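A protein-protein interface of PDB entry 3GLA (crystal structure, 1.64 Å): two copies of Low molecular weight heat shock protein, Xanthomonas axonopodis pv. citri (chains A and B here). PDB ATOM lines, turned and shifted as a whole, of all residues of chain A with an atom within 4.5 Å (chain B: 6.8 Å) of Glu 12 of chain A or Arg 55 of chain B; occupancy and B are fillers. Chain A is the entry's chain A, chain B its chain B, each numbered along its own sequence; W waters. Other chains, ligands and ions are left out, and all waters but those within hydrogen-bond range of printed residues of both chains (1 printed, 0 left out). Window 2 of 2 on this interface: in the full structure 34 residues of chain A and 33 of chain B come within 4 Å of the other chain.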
ATOM      1  N   ILE A   9      17.089 -10.922  18.240  1.00  0.00           N
ATOM      2  CA  ILE A   9      16.069  -9.956  18.596  1.00  0.00           C
ATOM      3  C   ILE A   9      16.209  -8.699  17.796  1.00  0.00           C
ATOM      4  O   ILE A   9      17.303  -8.217  17.713  1.00  0.00           O
ATOM      5  CB  ILE A   9      16.191  -9.575  20.071  1.00  0.00           C
ATOM      6  CG1 ILE A   9      15.990 -10.811  20.873  1.00  0.00           C
ATOM      7  CG2 ILE A   9      15.075  -8.610  20.466  1.00  0.00           C
ATOM      8  CD1 ILE A   9      16.282 -10.660  22.468  1.00  0.00           C
ATOM      9  N   LYS A  10      15.103  -8.210  17.234  1.00  0.00           N
ATOM     10  CA  LYS A  10      15.203  -7.028  16.483  1.00  0.00           C
ATOM     11  C   LYS A  10      14.142  -6.116  16.953  1.00  0.00           C
ATOM     12  O   LYS A  10      13.102  -6.486  17.369  1.00  0.00           O
ATOM     13  CB  LYS A  10      14.951  -7.477  15.004  1.00  0.00           C
ATOM     14  CG  LYS A  10      13.967  -6.874  14.238  1.00  0.00           C
ATOM     15  CD  LYS A  10      13.987  -7.195  12.778  1.00  0.00           C
ATOM     16  CE  LYS A  10      12.465  -7.726  12.622  1.00  0.00           C
ATOM     17  NZ  LYS A  10      12.269  -7.717  11.125  1.00  0.00           N
ATOM     18  N   GLU A  11      14.460  -4.865  16.913  1.00  0.00           N
ATOM     19  CA  GLU A  11      13.509  -3.794  17.193  1.00  0.00           C
ATOM     20  C   GLU A  11      13.308  -3.063  15.913  1.00  0.00           C
ATOM     21  O   GLU A  11      14.183  -2.374  15.338  1.00  0.00           O
ATOM     22  CB  GLU A  11      14.108  -2.853  18.251  1.00  0.00           C
ATOM     23  CG  GLU A  11      13.036  -1.751  18.533  1.00  0.00           C
ATOM     24  CD  GLU A  11      13.484  -0.744  19.590  1.00  0.00           C
ATOM     25  OE1 GLU A  11      14.431  -1.033  20.346  1.00  0.00           O
ATOM     26  OE2 GLU A  11      12.884   0.288  19.651  1.00  0.00           O
ATOM     27  N   GLU A  12      12.107  -3.230  15.393  1.00  0.00           N
ATOM     28  CA  GLU A  12      11.691  -2.425  14.257  1.00  0.00           C
ATOM     29  C   GLU A  12      11.060  -1.163  14.748  1.00  0.00           C
ATOM     30  O   GLU A  12      10.883  -0.933  15.923  1.00  0.00           O
ATOM     31  CB  GLU A  12      10.651  -3.219  13.435  1.00  0.00           C
ATOM     32  CG  GLU A  12      11.331  -4.306  12.703  1.00  0.00           C
ATOM     33  CD  GLU A  12      12.097  -3.930  11.474  1.00  0.00           C
ATOM     34  OE1 GLU A  12      12.783  -4.794  10.918  1.00  0.00           O
ATOM     35  OE2 GLU A  12      12.024  -2.747  11.056  1.00  0.00           O
ATOM     36  N   VAL A  13      10.575  -0.372  13.763  1.00  0.00           N
ATOM     37  CA  VAL A  13      10.041   0.854  14.210  1.00  0.00           C
ATOM     38  C   VAL A  13       8.868   0.718  15.090  1.00  0.00           C
ATOM     39  O   VAL A  13       8.702   1.385  16.048  1.00  0.00           O
ATOM     40  CB  VAL A  13       9.677   1.755  12.967  1.00  0.00           C
ATOM     41  CG1 VAL A  13       9.008   2.943  13.509  1.00  0.00           C
ATOM     42  CG2 VAL A  13      10.960   2.238  12.255  1.00  0.00           C
ATOM     43  N   ASN A  14       7.983  -0.255  14.746  1.00  0.00           N
ATOM     44  CA  ASN A  14       6.813  -0.319  15.542  1.00  0.00           C
ATOM     45  C   ASN A  14       6.560  -1.698  16.164  1.00  0.00           C
ATOM     46  O   ASN A  14       5.498  -1.916  16.755  1.00  0.00           O
ATOM     47  CB  ASN A  14       5.523   0.026  14.681  1.00  0.00           C
ATOM     48  CG  ASN A  14       5.357  -0.839  13.471  1.00  0.00           C
ATOM     49  OD1 ASN A  14       4.638  -0.464  12.461  1.00  0.00           O
ATOM     50  ND2 ASN A  14       5.939  -2.002  13.490  1.00  0.00           N
ATOM     51  N   HIS A  15       7.611  -2.523  16.197  1.00  0.00           N
ATOM     52  CA  HIS A  15       7.405  -3.787  16.870  1.00  0.00           C
ATOM     53  C   HIS A  15       8.776  -4.392  17.108  1.00  0.00           C
ATOM     54  O   HIS A  15       9.734  -3.987  16.467  1.00  0.00           O
ATOM     55  CB  HIS A  15       6.544  -4.774  16.059  1.00  0.00           C
ATOM     56  CG  HIS A  15       7.122  -5.188  14.766  1.00  0.00           C
ATOM     57  ND1 HIS A  15       7.220  -4.362  13.656  1.00  0.00           N
ATOM     58  CD2 HIS A  15       7.720  -6.354  14.429  1.00  0.00           C
ATOM     59  CE1 HIS A  15       7.778  -5.034  12.653  1.00  0.00           C
ATOM     60  NE2 HIS A  15       8.131  -6.232  13.108  1.00  0.00           N
ATOM     61  N   LYS A  96       5.175  -2.308  19.529  1.00  0.00           N
ATOM     62  CA  LYS A  96       5.487  -1.247  20.485  1.00  0.00           C
ATOM     63  C   LYS A  96       4.259  -0.470  20.873  1.00  0.00           C
ATOM     64  O   LYS A  96       3.266  -0.386  20.107  1.00  0.00           O
ATOM     65  CB  LYS A  96       6.443  -0.336  19.818  1.00  0.00           C
ATOM     66  CG  LYS A  96       7.769  -0.921  19.768  1.00  0.00           C
ATOM     67  CD  LYS A  96       8.565   0.274  19.093  1.00  0.00           C
ATOM     68  CE  LYS A  96       9.935  -0.073  19.045  1.00  0.00           C
ATOM     69  NZ  LYS A  96      10.659   0.881  18.209  1.00  0.00           N
ATOM     70  N   THR B  51      18.781  -9.161   7.308  1.00  0.00           N
ATOM     71  CA  THR B  51      17.979  -8.030   6.749  1.00  0.00           C
ATOM     72  C   THR B  51      17.848  -6.986   7.861  1.00  0.00           C
ATOM     73  O   THR B  51      17.426  -7.351   8.938  1.00  0.00           O
ATOM     74  CB  THR B  51      16.609  -8.502   6.377  1.00  0.00           C
ATOM     75  OG1 THR B  51      16.791  -9.475   5.342  1.00  0.00           O
ATOM     76  CG2 THR B  51      15.755  -7.349   5.830  1.00  0.00           C
ATOM     77  N   GLU B  52      18.181  -5.726   7.578  1.00  0.00           N
ATOM     78  CA  GLU B  52      17.951  -4.643   8.595  1.00  0.00           C
ATOM     79  C   GLU B  52      18.725  -5.072   9.845  1.00  0.00           C
ATOM     80  O   GLU B  52      18.170  -4.937  10.971  1.00  0.00           O
ATOM     81  CB  GLU B  52      16.504  -4.555   9.038  1.00  0.00           C
ATOM     82  CG  GLU B  52      15.478  -3.998   7.920  1.00  0.00           C
ATOM     83  CD  GLU B  52      15.965  -2.701   7.298  1.00  0.00           C
ATOM     84  OE1 GLU B  52      16.000  -2.636   6.045  1.00  0.00           O
ATOM     85  OE2 GLU B  52      16.341  -1.754   8.058  1.00  0.00           O
ATOM     86  N   THR B  53      19.977  -5.486   9.637  1.00  0.00           N
ATOM     87  CA  THR B  53      20.815  -6.071  10.720  1.00  0.00           C
ATOM     88  C   THR B  53      20.988  -5.058  11.825  1.00  0.00           C
ATOM     89  O   THR B  53      21.015  -5.396  13.033  1.00  0.00           O
ATOM     90  CB  THR B  53      22.180  -6.457  10.122  1.00  0.00           C
ATOM     91  OG1 THR B  53      21.933  -7.424   9.067  1.00  0.00           O
ATOM     92  CG2 THR B  53      23.033  -7.205  11.122  1.00  0.00           C
ATOM     93  N   GLU B  54      21.064  -3.780  11.454  1.00  0.00           N
ATOM     94  CA  GLU B  54      21.282  -2.758  12.427  1.00  0.00           C
ATOM     95  C   GLU B  54      20.087  -2.610  13.466  1.00  0.00           C
ATOM     96  O   GLU B  54      20.237  -2.043  14.496  1.00  0.00           O
ATOM     97  CB  GLU B  54      21.444  -1.414  11.666  1.00  0.00           C
ATOM     98  CG  GLU B  54      20.179  -0.853  11.074  1.00  0.00           C
ATOM     99  CD  GLU B  54      19.941  -1.489   9.676  1.00  0.00           C
ATOM    100  OE1 GLU B  54      18.794  -1.218   9.171  1.00  0.00           O
ATOM    101  OE2 GLU B  54      20.905  -2.258   9.165  1.00  0.00           O
ATOM    102  N   ARG B  55      18.922  -3.169  13.179  1.00  0.00           N
ATOM    103  CA  ARG B  55      17.792  -3.043  14.080  1.00  0.00           C
ATOM    104  C   ARG B  55      17.877  -4.198  15.088  1.00  0.00           C
ATOM    105  O   ARG B  55      17.048  -4.200  15.977  1.00  0.00           O
ATOM    106  CB  ARG B  55      16.520  -3.288  13.313  1.00  0.00           C
ATOM    107  CG  ARG B  55      16.442  -2.239  12.233  1.00  0.00           C
ATOM    108  CD  ARG B  55      15.051  -1.830  11.942  1.00  0.00           C
ATOM    109  NE  ARG B  55      14.995  -0.598  11.134  1.00  0.00           N
ATOM    110  CZ  ARG B  55      14.397  -0.485   9.940  1.00  0.00           C
ATOM    111  NH1 ARG B  55      14.470   0.710   9.339  1.00  0.00           N
ATOM    112  NH2 ARG B  55      13.692  -1.529   9.362  1.00  0.00           N
ATOM    113  N   PHE B  56      18.810  -5.148  14.917  1.00  0.00           N
ATOM    114  CA  PHE B  56      18.889  -6.274  15.889  1.00  0.00           C
ATOM    115  C   PHE B  56      19.628  -5.844  17.096  1.00  0.00           C
ATOM    116  O   PHE B  56      20.673  -5.194  16.991  1.00  0.00           O
ATOM    117  CB  PHE B  56      19.607  -7.450  15.263  1.00  0.00           C
ATOM    118  CG  PHE B  56      18.640  -8.215  14.374  1.00  0.00           C
ATOM    119  CD1 PHE B  56      18.119  -9.397  14.806  1.00  0.00           C
ATOM    120  CD2 PHE B  56      18.312  -7.661  13.132  1.00  0.00           C
ATOM    121  CE1 PHE B  56      17.188 -10.145  13.984  1.00  0.00           C
ATOM    122  CE2 PHE B  56      17.389  -8.367  12.337  1.00  0.00           C
ATOM    123  CZ  PHE B  56      16.818  -9.535  12.772  1.00  0.00           C
ATOM    124  N   SER B  57      19.044  -6.131  18.251  1.00  0.00           N
ATOM    125  CA  SER B  57      19.774  -5.895  19.480  1.00  0.00           C
ATOM    126  C   SER B  57      20.415  -7.121  19.949  1.00  0.00           C
ATOM    127  O   SER B  57      21.187  -7.072  20.949  1.00  0.00           O
ATOM    128  CB  SER B  57      18.737  -5.413  20.497  1.00  0.00           C
ATOM    129  OG  SER B  57      17.823  -6.521  20.705  1.00  0.00           O
ATOM    130  N   ARG B  58      20.164  -8.259  19.301  1.00  0.00           N
ATOM    131  CA  ARG B  58      20.848  -9.469  19.663  1.00  0.00           C
ATOM    132  C   ARG B  58      20.856 -10.301  18.456  1.00  0.00           C
ATOM    133  O   ARG B  58      19.830 -10.508  17.806  1.00  0.00           O
ATOM    134  CB  ARG B  58      20.080 -10.238  20.769  1.00  0.00           C
ATOM    135  CG  ARG B  58      20.716 -11.547  21.116  1.00  0.00           C
ATOM    136  CD  ARG B  58      19.811 -12.192  22.182  1.00  0.00           C
ATOM    137  NE  ARG B  58      20.462 -13.409  22.493  1.00  0.00           N
ATOM    138  CZ  ARG B  58      21.347 -13.535  23.446  1.00  0.00           C
ATOM    139  NH1 ARG B  58      21.971 -14.710  23.602  1.00  0.00           N
ATOM    140  NH2 ARG B  58      21.674 -12.421  24.192  1.00  0.00           N
HETATM  141  O   HOH W   1      14.886  -8.737   9.611  1.00  0.00           O
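O of Ile 9 of chain A lies within hydrogen-bond range of N of Ser 57 of chain B (2.8 Å).
The backbone NH of Ile 9 of chain A lies within hydrogen-bond range of the backbone carbonyl oxygen of Arg 58 of chain B (2.8 Å).
The backbone carbonyl oxygen of Arg 55 of chain B is in hydrogen-bond range of the backbone NH of Glu 11 of chain A (2.8 Å).
The side-chain carboxylate of Glu 12 of chain A is in salt-bridge range of the guanidinium group of Arg 55 of chain B, at 2.7 Å.
The side-chain amino group (NZ) of Lys 10 of chain A lies within salt-bridge range of the side-chain carboxylate (OE1) of Glu 12 of chain A, 3.0 Å away.
The side-chain amino group (NZ) of Lys 96 of chain A is in salt-bridge range of the side-chain carboxylate (OE2) of Glu 11 of chain A, 2.7 Å away.
The side-chain amino group of Lys 96 of chain A is in hydrogen-bond range of the backbone carbonyl oxygen of Glu 12 of chain A, at 2.9 Å.
The guanidinium group of Arg 55 of chain B lies within salt-bridge range of the side-chain carboxylate of Glu 52 of chain B (3.0 Å).
Ile 9 of chain A touches Phe 56 of chain B (O to CA, 3.1 Å).
Arg 55 of chain B touches Lys 10 of chain A.
CZ of Phe 56 of chain B touches CB of Lys 10 of chain A, at 3.6 Å.
Of the printed residues of chain B, Ile 9 of chain A touches Phe 56 (3.1 Å), Ser 57 (2.8 Å) and Arg 58 (2.8 Å).
Of the printed residues of chain B, Glu 11 of chain A touches Arg 55.
Glu 12 of chain A touches just one residue of chain B: Arg 55 (2.7 Å).
Glu 52 of chain B touches none of the printed residues of chain A.
Arg 55 of chain B touches just these residues of chain A: Lys 10, Glu 11 and Glu 12.
Of the printed residues of chain A, Phe 56 of chain B touches Ile 9 (3.1 Å) and Lys 10 (3.6 Å).
The nearest residue of chain A that does not touch Arg 55 of chain B is Ile 9 of chain A (4.4 Å).
Hydrophobic or aromatic side chains of chain A that line the printed part of chain B: Ile 9.
Of the 8 printed residues of chain B, 4 touch a printed residue of chain A.
Hydrophobic or aromatic side chains of chain B that line the printed part of chain A: Phe 56.
No position is printed for both chains.
Water W1 bridges O of Thr 51 of chain B (3.0 Å) and NZ of Lys 10 of chain A (3.2 Å).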
